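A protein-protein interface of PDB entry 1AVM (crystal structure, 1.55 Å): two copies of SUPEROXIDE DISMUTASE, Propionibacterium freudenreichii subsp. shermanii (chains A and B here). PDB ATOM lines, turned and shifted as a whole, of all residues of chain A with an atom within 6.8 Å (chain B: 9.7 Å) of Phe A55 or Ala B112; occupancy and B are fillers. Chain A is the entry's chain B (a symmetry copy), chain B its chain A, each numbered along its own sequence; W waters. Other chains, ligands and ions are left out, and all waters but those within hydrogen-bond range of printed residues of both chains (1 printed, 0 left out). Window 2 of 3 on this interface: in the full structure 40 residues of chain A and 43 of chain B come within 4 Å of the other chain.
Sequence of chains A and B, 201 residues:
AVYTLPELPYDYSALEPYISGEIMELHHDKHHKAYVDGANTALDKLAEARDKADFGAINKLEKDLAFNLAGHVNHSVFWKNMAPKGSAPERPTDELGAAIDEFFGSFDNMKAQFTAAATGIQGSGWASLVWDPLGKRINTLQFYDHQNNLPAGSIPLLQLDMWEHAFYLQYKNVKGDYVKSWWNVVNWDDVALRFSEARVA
O of Ala B117 is in hydrogen-bond range of NE2 of Gln B142 (2.8 Å). OE1 of Gln B113 sits at hydrogen-bond distance from OG1 of Thr B140 (2.6 Å). The side-chain amide nitrogen (ND2) of Asn B109 sits close to the backbone carbonyl oxygen (O) of Phe B104 (3.1 Å).
Water W1 bridges OE1 of Gln B142 and O of Asn A59.
NE2 of Gln B113 sits close to NE of Arg A50 (3.1 Å). The backbone carbonyl oxygen (O) of Gly B120 lies within hydrogen-bond range of the side-chain amide nitrogen (ND2) of Asn A59, at 2.7 Å. O of Phe B104 sits at hydrogen-bond distance from NH1 of Arg A50 (3.4 Å). The side-chain amide nitrogen (NE2) of Gln B142 is in hydrogen-bond range of the side-chain amide oxygen (OD1) of Asn A59 (2.9 Å).
No position is printed for both chains. Of the 9 pairs that touch across the chains among the printed residues, none has its exchanged pair printed and touching as well.
No residue of chain B comes within 4 Å of Ala A53. No residue of chain B comes within 4 Å of Asp A54. Phe A55 touches just these residues of chain B: Ala B112 (3.7 Å), Gln B113 (3.7 Å) and Ala B116 (3.5 Å). No residue of chain B comes within 4 Å of Ala A57. Of chain A, only Phe A55 (3.7 Å) comes within 4 Å of Ala B112. Of the printed residues of chain A, Gln B113 touches Arg A50 and Phe A55. Of the printed residues of chain A, Ala B117 touches Ile A58 (3.9 Å). Of the printed residues of chain A, Gly B120 touches Asn A59 (2.7 Å).
Of the 13 printed residues of chain A, 4 touch a printed residue of chain B. Printed residues of chain A that touch a printed residue of chain B: Arg A50, Phe A55, Ile A58 and Asn A59. Hydrophobic or aromatic side chains of chain A that line the printed part of chain B: Phe A55 and Ile A58. Along chain B the printed residues that touch a printed residue of chain A span positions 104 to 142. Among the printed residues, no Asp or Glu carboxylate lies within 4 Å of a Lys or Arg side-chain nitrogen of the other chain.
Among the printed residues, merely in contact across the chains: Phe A55 with Ala B112 (3.7 Å), Phe A55 with Gln B113 (3.7 Å), Phe A55 with Ala B116 (3.5 Å), Ile A58 with Ala B116 (3.7 Å) and Ile A58 with Ala B117 (3.9 Å).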
ATOM      1  N   LEU A  46      -4.381  -0.938   5.496  1.00  0.00           N
ATOM      2  CA  LEU A  46      -3.925  -0.110   4.384  1.00  0.00           C
ATOM      3  C   LEU A  46      -2.561   0.496   4.684  1.00  0.00           C
ATOM      4  O   LEU A  46      -1.711   0.591   3.801  1.00  0.00           O
ATOM      5  CB  LEU A  46      -4.946   0.989   4.081  1.00  0.00           C
ATOM      6  CG  LEU A  46      -6.198   0.523   3.334  1.00  0.00           C
ATOM      7  CD1 LEU A  46      -7.290   1.579   3.411  1.00  0.00           C
ATOM      8  CD2 LEU A  46      -5.847   0.202   1.889  1.00  0.00           C
ATOM      9  N   ALA A  49      -0.034  -2.133   4.254  1.00  0.00           N
ATOM     10  CA  ALA A  49       0.155  -2.389   2.830  1.00  0.00           C
ATOM     11  C   ALA A  49       1.152  -1.380   2.265  1.00  0.00           C
ATOM     12  O   ALA A  49       1.984  -1.723   1.428  1.00  0.00           O
ATOM     13  CB  ALA A  49      -1.174  -2.293   2.091  1.00  0.00           C
ATOM     14  N   ARG A  50       1.073  -0.142   2.752  1.00  0.00           N
ATOM     15  CA  ARG A  50       1.966   0.933   2.322  1.00  0.00           C
ATOM     16  C   ARG A  50       3.409   0.706   2.777  1.00  0.00           C
ATOM     17  O   ARG A  50       4.346   0.933   2.012  1.00  0.00           O
ATOM     18  CB  ARG A  50       1.466   2.284   2.839  1.00  0.00           C
ATOM     19  CG  ARG A  50       0.564   3.030   1.871  1.00  0.00           C
ATOM     20  CD  ARG A  50       0.106   4.364   2.449  1.00  0.00           C
ATOM     21  NE  ARG A  50      -0.995   4.206   3.398  1.00  0.00           N
ATOM     22  CZ  ARG A  50      -0.977   4.631   4.658  1.00  0.00           C
ATOM     23  NH1 ARG A  50       0.089   5.245   5.154  1.00  0.00           N
ATOM     24  NH2 ARG A  50      -2.039   4.448   5.426  1.00  0.00           N
ATOM     25  N   ASP A  51       3.577   0.270   4.024  1.00  0.00           N
ATOM     26  CA  ASP A  51       4.902   0.004   4.581  1.00  0.00           C
ATOM     27  C   ASP A  51       5.577  -1.159   3.859  1.00  0.00           C
ATOM     28  O   ASP A  51       6.742  -1.066   3.471  1.00  0.00           O
ATOM     29  CB  ASP A  51       4.805  -0.315   6.076  1.00  0.00           C
ATOM     30  CG  ASP A  51       4.499   0.908   6.924  1.00  0.00           C
ATOM     31  OD1 ASP A  51       3.623   1.714   6.537  1.00  0.00           O
ATOM     32  OD2 ASP A  51       5.136   1.058   7.988  1.00  0.00           O
ATOM     33  N   LYS A  52       4.831  -2.247   3.679  1.00  0.00           N
ATOM     34  CA  LYS A  52       5.334  -3.445   3.011  1.00  0.00           C
ATOM     35  C   LYS A  52       5.378  -3.255   1.494  1.00  0.00           C
ATOM     36  O   LYS A  52       5.970  -4.065   0.778  1.00  0.00           O
ATOM     37  CB  LYS A  52       4.448  -4.651   3.353  1.00  0.00           C
ATOM     38  CG  LYS A  52       4.186  -4.843   4.848  1.00  0.00           C
ATOM     39  CD  LYS A  52       5.407  -5.353   5.608  1.00  0.00           C
ATOM     40  CE  LYS A  52       5.440  -6.876   5.659  1.00  0.00           C
ATOM     41  NZ  LYS A  52       6.597  -7.387   6.454  1.00  0.00           N
ATOM     42  N   ALA A  53       4.741  -2.186   1.018  1.00  0.00           N
ATOM     43  CA  ALA A  53       4.680  -1.861  -0.407  1.00  0.00           C
ATOM     44  C   ALA A  53       4.014  -2.968  -1.222  1.00  0.00           C
ATOM     45  O   ALA A  53       4.350  -3.188  -2.387  1.00  0.00           O
ATOM     46  CB  ALA A  53       6.074  -1.553  -0.949  1.00  0.00           C
ATOM     47  N   ASP A  54       3.076  -3.671  -0.592  1.00  0.00           N
ATOM     48  CA  ASP A  54       2.349  -4.755  -1.244  1.00  0.00           C
ATOM     49  C   ASP A  54       0.856  -4.453  -1.196  1.00  0.00           C
ATOM     50  O   ASP A  54       0.241  -4.474  -0.129  1.00  0.00           O
ATOM     51  CB  ASP A  54       2.633  -6.089  -0.548  1.00  0.00           C
ATOM     52  CG  ASP A  54       2.130  -7.276  -1.344  1.00  0.00           C
ATOM     53  OD1 ASP A  54       0.935  -7.617  -1.226  1.00  0.00           O
ATOM     54  OD2 ASP A  54       2.932  -7.866  -2.099  1.00  0.00           O
ATOM     55  N   PHE A  55       0.281  -4.169  -2.362  1.00  0.00           N
ATOM     56  CA  PHE A  55      -1.138  -3.847  -2.462  1.00  0.00           C
ATOM     57  C   PHE A  55      -1.938  -4.975  -3.096  1.00  0.00           C
ATOM     58  O   PHE A  55      -2.908  -4.731  -3.814  1.00  0.00           O
ATOM     59  CB  PHE A  55      -1.329  -2.552  -3.256  1.00  0.00           C
ATOM     60  CG  PHE A  55      -0.653  -1.363  -2.641  1.00  0.00           C
ATOM     61  CD1 PHE A  55      -1.263  -0.657  -1.611  1.00  0.00           C
ATOM     62  CD2 PHE A  55       0.607  -0.961  -3.077  1.00  0.00           C
ATOM     63  CE1 PHE A  55      -0.624   0.431  -1.017  1.00  0.00           C
ATOM     64  CE2 PHE A  55       1.257   0.124  -2.493  1.00  0.00           C
ATOM     65  CZ  PHE A  55       0.640   0.822  -1.460  1.00  0.00           C
ATOM     66  N   GLY A  56      -1.535  -6.212  -2.815  1.00  0.00           N
ATOM     67  CA  GLY A  56      -2.226  -7.362  -3.370  1.00  0.00           C
ATOM     68  C   GLY A  56      -3.683  -7.457  -2.954  1.00  0.00           C
ATOM     69  O   GLY A  56      -4.524  -7.909  -3.728  1.00  0.00           O
ATOM     70  N   ALA A  57      -3.990  -6.999  -1.743  1.00  0.00           N
ATOM     71  CA  ALA A  57      -5.354  -7.050  -1.226  1.00  0.00           C
ATOM     72  C   ALA A  57      -6.069  -5.700  -1.271  1.00  0.00           C
ATOM     73  O   ALA A  57      -7.018  -5.476  -0.520  1.00  0.00           O
ATOM     74  CB  ALA A  57      -5.346  -7.589   0.200  1.00  0.00           C
ATOM     75  N   ILE A  58      -5.643  -4.823  -2.177  1.00  0.00           N
ATOM     76  CA  ILE A  58      -6.245  -3.496  -2.293  1.00  0.00           C
ATOM     77  C   ILE A  58      -7.760  -3.521  -2.537  1.00  0.00           C
ATOM     78  O   ILE A  58      -8.491  -2.719  -1.953  1.00  0.00           O
ATOM     79  CB  ILE A  58      -5.530  -2.632  -3.376  1.00  0.00           C
ATOM     80  CG1 ILE A  58      -6.008  -1.177  -3.304  1.00  0.00           C
ATOM     81  CG2 ILE A  58      -5.753  -3.208  -4.766  1.00  0.00           C
ATOM     82  CD1 ILE A  58      -5.573  -0.439  -2.050  1.00  0.00           C
ATOM     83  N   ASN A  59      -8.236  -4.455  -3.361  1.00  0.00           N
ATOM     84  CA  ASN A  59      -9.671  -4.552  -3.648  1.00  0.00           C
ATOM     85  C   ASN A  59     -10.473  -4.890  -2.393  1.00  0.00           C
ATOM     86  O   ASN A  59     -11.527  -4.301  -2.133  1.00  0.00           O
ATOM     87  CB  ASN A  59      -9.937  -5.586  -4.744  1.00  0.00           C
ATOM     88  CG  ASN A  59      -9.446  -5.132  -6.114  1.00  0.00           C
ATOM     89  OD1 ASN A  59      -9.072  -3.972  -6.299  1.00  0.00           O
ATOM     90  ND2 ASN A  59      -9.450  -6.044  -7.080  1.00  0.00           N
ATOM     91  N   LEU A  61      -9.447  -4.451   0.806  1.00  0.00           N
ATOM     92  CA  LEU A  61      -9.295  -3.358   1.757  1.00  0.00           C
ATOM     93  C   LEU A  61     -10.143  -2.134   1.445  1.00  0.00           C
ATOM     94  O   LEU A  61     -10.674  -1.506   2.359  1.00  0.00           O
ATOM     95  CB  LEU A  61      -7.823  -2.981   1.908  1.00  0.00           C
ATOM     96  CG  LEU A  61      -6.934  -4.120   2.421  1.00  0.00           C
ATOM     97  CD1 LEU A  61      -5.509  -3.637   2.584  1.00  0.00           C
ATOM     98  CD2 LEU A  61      -7.465  -4.652   3.740  1.00  0.00           C
ATOM     99  N   ILE B 100      -1.074  15.014   2.711  1.00  0.00           N
ATOM    100  CA  ILE B 100      -0.801  13.748   2.034  1.00  0.00           C
ATOM    101  C   ILE B 100       0.302  12.994   2.781  1.00  0.00           C
ATOM    102  O   ILE B 100       0.228  11.775   2.944  1.00  0.00           O
ATOM    103  CB  ILE B 100      -0.400  13.972   0.559  1.00  0.00           C
ATOM    104  CG1 ILE B 100      -1.613  14.471  -0.234  1.00  0.00           C
ATOM    105  CG2 ILE B 100       0.156  12.688  -0.045  1.00  0.00           C
ATOM    106  CD1 ILE B 100      -1.321  14.801  -1.680  1.00  0.00           C
ATOM    107  N   PHE B 104      -0.523   9.366   4.403  1.00  0.00           N
ATOM    108  CA  PHE B 104       0.036   8.334   3.529  1.00  0.00           C
ATOM    109  C   PHE B 104       1.526   8.096   3.755  1.00  0.00           C
ATOM    110  O   PHE B 104       2.090   7.133   3.236  1.00  0.00           O
ATOM    111  CB  PHE B 104      -0.204   8.688   2.055  1.00  0.00           C
ATOM    112  CG  PHE B 104      -1.656   8.774   1.678  1.00  0.00           C
ATOM    113  CD1 PHE B 104      -2.341   7.649   1.232  1.00  0.00           C
ATOM    114  CD2 PHE B 104      -2.340   9.982   1.773  1.00  0.00           C
ATOM    115  CE1 PHE B 104      -3.686   7.723   0.889  1.00  0.00           C
ATOM    116  CE2 PHE B 104      -3.684  10.070   1.434  1.00  0.00           C
ATOM    117  CZ  PHE B 104      -4.361   8.939   0.990  1.00  0.00           C
ATOM    118  N   SER B 106       4.069   9.601   2.553  1.00  0.00           N
ATOM    119  CA  SER B 106       4.765  10.351   1.517  1.00  0.00           C
ATOM    120  C   SER B 106       3.912  10.417   0.259  1.00  0.00           C
ATOM    121  O   SER B 106       2.915   9.701   0.133  1.00  0.00           O
ATOM    122  CB  SER B 106       6.112   9.696   1.186  1.00  0.00           C
ATOM    123  OG  SER B 106       5.946   8.392   0.647  1.00  0.00           O
ATOM    124  N   PHE B 107       4.312  11.281  -0.671  1.00  0.00           N
ATOM    125  CA  PHE B 107       3.599  11.429  -1.932  1.00  0.00           C
ATOM    126  C   PHE B 107       3.698  10.132  -2.730  1.00  0.00           C
ATOM    127  O   PHE B 107       2.729   9.711  -3.362  1.00  0.00           O
ATOM    128  CB  PHE B 107       4.183  12.586  -2.751  1.00  0.00           C
ATOM    129  CG  PHE B 107       3.549  12.750  -4.102  1.00  0.00           C
ATOM    130  CD1 PHE B 107       2.191  13.029  -4.217  1.00  0.00           C
ATOM    131  CD2 PHE B 107       4.301  12.606  -5.261  1.00  0.00           C
ATOM    132  CE1 PHE B 107       1.593  13.159  -5.467  1.00  0.00           C
ATOM    133  CE2 PHE B 107       3.714  12.736  -6.515  1.00  0.00           C
ATOM    134  CZ  PHE B 107       2.356  13.014  -6.618  1.00  0.00           C
ATOM    135  N   ASP B 108       4.873   9.508  -2.696  1.00  0.00           N
ATOM    136  CA  ASP B 108       5.098   8.264  -3.419  1.00  0.00           C
ATOM    137  C   ASP B 108       4.209   7.130  -2.918  1.00  0.00           C
ATOM    138  O   ASP B 108       3.742   6.310  -3.709  1.00  0.00           O
ATOM    139  CB  ASP B 108       6.574   7.869  -3.360  1.00  0.00           C
ATOM    140  CG  ASP B 108       7.429   8.684  -4.314  1.00  0.00           C
ATOM    141  OD1 ASP B 108       7.513   9.916  -4.142  1.00  0.00           O
ATOM    142  OD2 ASP B 108       8.004   8.093  -5.250  1.00  0.00           O
ATOM    143  N   ASN B 109       3.969   7.097  -1.608  1.00  0.00           N
ATOM    144  CA  ASN B 109       3.112   6.076  -1.011  1.00  0.00           C
ATOM    145  C   ASN B 109       1.667   6.275  -1.458  1.00  0.00           C
ATOM    146  O   ASN B 109       0.958   5.309  -1.749  1.00  0.00           O
ATOM    147  CB  ASN B 109       3.198   6.129   0.514  1.00  0.00           C
ATOM    148  CG  ASN B 109       4.414   5.403   1.057  1.00  0.00           C
ATOM    149  OD1 ASN B 109       5.186   4.805   0.302  1.00  0.00           O
ATOM    150  ND2 ASN B 109       4.582   5.436   2.374  1.00  0.00           N
ATOM    151  N   MET B 110       1.243   7.534  -1.514  1.00  0.00           N
ATOM    152  CA  MET B 110      -0.109   7.874  -1.940  1.00  0.00           C
ATOM    153  C   MET B 110      -0.304   7.460  -3.396  1.00  0.00           C
ATOM    154  O   MET B 110      -1.326   6.873  -3.743  1.00  0.00           O
ATOM    155  CB  MET B 110      -0.354   9.376  -1.766  1.00  0.00           C
ATOM    156  CG  MET B 110      -1.768   9.847  -2.100  1.00  0.00           C
ATOM    157  SD  MET B 110      -2.110   9.961  -3.873  1.00  0.00           S
ATOM    158  CE  MET B 110      -1.609  11.640  -4.199  1.00  0.00           C
ATOM    159  N   LYS B 111       0.689   7.749  -4.236  1.00  0.00           N
ATOM    160  CA  LYS B 111       0.628   7.398  -5.653  1.00  0.00           C
ATOM    161  C   LYS B 111       0.535   5.897  -5.853  1.00  0.00           C
ATOM    162  O   LYS B 111      -0.250   5.428  -6.672  1.00  0.00           O
ATOM    163  CB  LYS B 111       1.850   7.923  -6.411  1.00  0.00           C
ATOM    164  CG  LYS B 111       1.679   9.312  -6.989  1.00  0.00           C
ATOM    165  CD  LYS B 111       2.855   9.687  -7.885  1.00  0.00           C
ATOM    166  CE  LYS B 111       2.992   8.741  -9.069  1.00  0.00           C
ATOM    167  NZ  LYS B 111       4.074   9.181  -9.998  1.00  0.00           N
ATOM    168  N   ALA B 112       1.342   5.151  -5.106  1.00  0.00           N
ATOM    169  CA  ALA B 112       1.347   3.696  -5.210  1.00  0.00           C
ATOM    170  C   ALA B 112      -0.006   3.103  -4.817  1.00  0.00           C
ATOM    171  O   ALA B 112      -0.519   2.219  -5.502  1.00  0.00           O
ATOM    172  CB  ALA B 112       2.458   3.109  -4.349  1.00  0.00           C
ATOM    173  N   GLN B 113      -0.585   3.604  -3.728  1.00  0.00           N
ATOM    174  CA  GLN B 113      -1.880   3.119  -3.258  1.00  0.00           C
ATOM    175  C   GLN B 113      -2.993   3.486  -4.234  1.00  0.00           C
ATOM    176  O   GLN B 113      -3.836   2.650  -4.560  1.00  0.00           O
ATOM    177  CB  GLN B 113      -2.196   3.670  -1.862  1.00  0.00           C
ATOM    178  CG  GLN B 113      -3.501   3.141  -1.272  1.00  0.00           C
ATOM    179  CD  GLN B 113      -3.708   3.548   0.177  1.00  0.00           C
ATOM    180  OE1 GLN B 113      -4.786   4.013   0.556  1.00  0.00           O
ATOM    181  NE2 GLN B 113      -2.689   3.348   1.001  1.00  0.00           N
ATOM    182  N   PHE B 114      -2.965   4.728  -4.717  1.00  0.00           N
ATOM    183  CA  PHE B 114      -3.959   5.235  -5.664  1.00  0.00           C
ATOM    184  C   PHE B 114      -3.887   4.458  -6.978  1.00  0.00           C
ATOM    185  O   PHE B 114      -4.915   4.119  -7.568  1.00  0.00           O
ATOM    186  CB  PHE B 114      -3.720   6.732  -5.919  1.00  0.00           C
ATOM    187  CG  PHE B 114      -4.806   7.407  -6.723  1.00  0.00           C
ATOM    188  CD1 PHE B 114      -4.804   7.350  -8.114  1.00  0.00           C
ATOM    189  CD2 PHE B 114      -5.817   8.123  -6.086  1.00  0.00           C
ATOM    190  CE1 PHE B 114      -5.792   7.997  -8.859  1.00  0.00           C
ATOM    191  CE2 PHE B 114      -6.807   8.772  -6.821  1.00  0.00           C
ATOM    192  CZ  PHE B 114      -6.793   8.709  -8.211  1.00  0.00           C
ATOM    193  N   THR B 115      -2.667   4.171  -7.422  1.00  0.00           N
ATOM    194  CA  THR B 115      -2.452   3.431  -8.662  1.00  0.00           C
ATOM    195  C   THR B 115      -2.927   1.984  -8.528  1.00  0.00           C
ATOM    196  O   THR B 115      -3.566   1.454  -9.433  1.00  0.00           O
ATOM    197  CB  THR B 115      -0.966   3.455  -9.075  1.00  0.00           C
ATOM    198  OG1 THR B 115      -0.552   4.813  -9.274  1.00  0.00           O
ATOM    199  CG2 THR B 115      -0.744   2.663 -10.361  1.00  0.00           C
ATOM    200  N   ALA B 116      -2.630   1.362  -7.393  1.00  0.00           N
ATOM    201  CA  ALA B 116      -3.042  -0.017  -7.152  1.00  0.00           C
ATOM    202  C   ALA B 116      -4.563  -0.100  -7.155  1.00  0.00           C
ATOM    203  O   ALA B 116      -5.144  -1.023  -7.726  1.00  0.00           O
ATOM    204  CB  ALA B 116      -2.487  -0.508  -5.825  1.00  0.00           C
ATOM    205  N   ALA B 117      -5.204   0.893  -6.545  1.00  0.00           N
ATOM    206  CA  ALA B 117      -6.662   0.941  -6.480  1.00  0.00           C
ATOM    207  C   ALA B 117      -7.262   1.148  -7.869  1.00  0.00           C
ATOM    208  O   ALA B 117      -8.317   0.601  -8.186  1.00  0.00           O
ATOM    209  CB  ALA B 117      -7.112   2.056  -5.539  1.00  0.00           C
ATOM    210  N   ALA B 118      -6.565   1.916  -8.702  1.00  0.00           N
ATOM    211  CA  ALA B 118      -7.026   2.212 -10.053  1.00  0.00           C
ATOM    212  C   ALA B 118      -6.939   1.034 -11.017  1.00  0.00           C
ATOM    213  O   ALA B 118      -7.875   0.778 -11.770  1.00  0.00           O
ATOM    214  CB  ALA B 118      -6.256   3.402 -10.617  1.00  0.00           C
ATOM    215  N   THR B 119      -5.824   0.314 -10.979  1.00  0.00           N
ATOM    216  CA  THR B 119      -5.607  -0.814 -11.882  1.00  0.00           C
ATOM    217  C   THR B 119      -6.245  -2.139 -11.453  1.00  0.00           C
ATOM    218  O   THR B 119      -6.439  -3.034 -12.281  1.00  0.00           O
ATOM    219  CB  THR B 119      -4.098  -1.045 -12.135  1.00  0.00           C
ATOM    220  OG1 THR B 119      -3.439  -1.332 -10.895  1.00  0.00           O
ATOM    221  CG2 THR B 119      -3.467   0.192 -12.758  1.00  0.00           C
ATOM    222  N   GLY B 120      -6.597  -2.248 -10.175  1.00  0.00           N
ATOM    223  CA  GLY B 120      -7.187  -3.477  -9.673  1.00  0.00           C
ATOM    224  C   GLY B 120      -8.697  -3.606  -9.747  1.00  0.00           C
ATOM    225  O   GLY B 120      -9.239  -4.657  -9.406  1.00  0.00           O
ATOM    226  N   ILE B 121      -9.378  -2.562 -10.214  1.00  0.00           N
ATOM    227  CA  ILE B 121     -10.836  -2.580 -10.302  1.00  0.00           C
ATOM    228  C   ILE B 121     -11.401  -3.713 -11.159  1.00  0.00           C
ATOM    229  O   ILE B 121     -10.965  -3.942 -12.287  1.00  0.00           O
ATOM    230  CB  ILE B 121     -11.392  -1.234 -10.818  1.00  0.00           C
ATOM    231  CG1 ILE B 121     -10.895  -0.092  -9.932  1.00  0.00           C
ATOM    232  CG2 ILE B 121     -12.919  -1.250 -10.798  1.00  0.00           C
ATOM    233  CD1 ILE B 121     -11.290   1.283 -10.422  1.00  0.00           C
ATOM    234  N   ALA B 127     -10.790   5.565  -9.247  1.00  0.00           N
ATOM    235  CA  ALA B 127      -9.807   5.577  -8.173  1.00  0.00           C
ATOM    236  C   ALA B 127     -10.083   6.973  -7.627  1.00  0.00           C
ATOM    237  O   ALA B 127     -10.162   7.934  -8.396  1.00  0.00           O
ATOM    238  CB  ALA B 127      -8.402   5.486  -8.727  1.00  0.00           C
ATOM    239  N   LEU B 129      -9.415  10.001  -4.410  1.00  0.00           N
ATOM    240  CA  LEU B 129      -8.770  10.543  -3.226  1.00  0.00           C
ATOM    241  C   LEU B 129      -9.863  11.431  -2.639  1.00  0.00           C
ATOM    242  O   LEU B 129     -10.284  12.399  -3.274  1.00  0.00           O
ATOM    243  CB  LEU B 129      -7.556  11.387  -3.626  1.00  0.00           C
ATOM    244  CG  LEU B 129      -6.604  11.823  -2.511  1.00  0.00           C
ATOM    245  CD1 LEU B 129      -5.910  10.599  -1.932  1.00  0.00           C
ATOM    246  CD2 LEU B 129      -5.578  12.805  -3.062  1.00  0.00           C
ATOM    247  N   THR B 140      -8.238   6.859   0.241  1.00  0.00           N
ATOM    248  CA  THR B 140      -8.390   6.494  -1.158  1.00  0.00           C
ATOM    249  C   THR B 140      -9.574   5.535  -1.180  1.00  0.00           C
ATOM    250  O   THR B 140      -9.717   4.692  -0.290  1.00  0.00           O
ATOM    251  CB  THR B 140      -7.159   5.773  -1.750  1.00  0.00           C
ATOM    252  OG1 THR B 140      -6.839   4.623  -0.957  1.00  0.00           O
ATOM    253  CG2 THR B 140      -5.968   6.715  -1.824  1.00  0.00           C
ATOM    254  N   GLN B 142     -12.244   3.163  -3.924  1.00  0.00           N
ATOM    255  CA  GLN B 142     -12.358   2.528  -5.225  1.00  0.00           C
ATOM    256  C   GLN B 142     -13.846   2.429  -5.546  1.00  0.00           C
ATOM    257  O   GLN B 142     -14.545   1.576  -4.999  1.00  0.00           O
ATOM    258  CB  GLN B 142     -11.729   1.131  -5.174  1.00  0.00           C
ATOM    259  CG  GLN B 142     -11.622   0.422  -6.510  1.00  0.00           C
ATOM    260  CD  GLN B 142     -11.130  -1.010  -6.368  1.00  0.00           C
ATOM    261  OE1 GLN B 142     -11.891  -1.903  -5.987  1.00  0.00           O
ATOM    262  NE2 GLN B 142      -9.855  -1.235  -6.666  1.00  0.00           N
ATOM    263  N   VAL B 179      -2.632   5.054 -16.575  1.00  0.00           N
ATOM    264  CA  VAL B 179      -2.451   5.632 -15.244  1.00  0.00           C
ATOM    265  C   VAL B 179      -1.112   6.370 -15.133  1.00  0.00           C
ATOM    266  O   VAL B 179      -1.054   7.468 -14.580  1.00  0.00           O
ATOM    267  CB  VAL B 179      -2.553   4.557 -14.136  1.00  0.00           C
ATOM    268  CG1 VAL B 179      -2.350   5.189 -12.769  1.00  0.00           C
ATOM    269  CG2 VAL B 179      -3.914   3.870 -14.197  1.00  0.00           C
ATOM    270  N   TRP B 183      -0.778  10.773 -14.537  1.00  0.00           N
ATOM    271  CA  TRP B 183      -0.117  11.520 -13.469  1.00  0.00           C
ATOM    272  C   TRP B 183       0.529  12.815 -13.974  1.00  0.00           C
ATOM    273  O   TRP B 183       0.639  13.790 -13.228  1.00  0.00           O
ATOM    274  CB  TRP B 183       0.927  10.652 -12.760  1.00  0.00           C
ATOM    275  CG  TRP B 183       0.330   9.617 -11.844  1.00  0.00           C
ATOM    276  CD1 TRP B 183       0.379   8.259 -11.997  1.00  0.00           C
ATOM    277  CD2 TRP B 183      -0.409   9.855 -10.634  1.00  0.00           C
ATOM    278  NE1 TRP B 183      -0.280   7.639 -10.961  1.00  0.00           N
ATOM    279  CE2 TRP B 183      -0.776   8.593 -10.112  1.00  0.00           C
ATOM    280  CE3 TRP B 183      -0.797  11.012  -9.942  1.00  0.00           C
ATOM    281  CZ2 TRP B 183      -1.510   8.454  -8.928  1.00  0.00           C
ATOM    282  CZ3 TRP B 183      -1.532  10.871  -8.761  1.00  0.00           C
ATOM    283  CH2 TRP B 183      -1.880   9.599  -8.270  1.00  0.00           C
HETATM  284  O   HOH W   1     -12.943  -2.490  -3.580  1.00  0.00           O
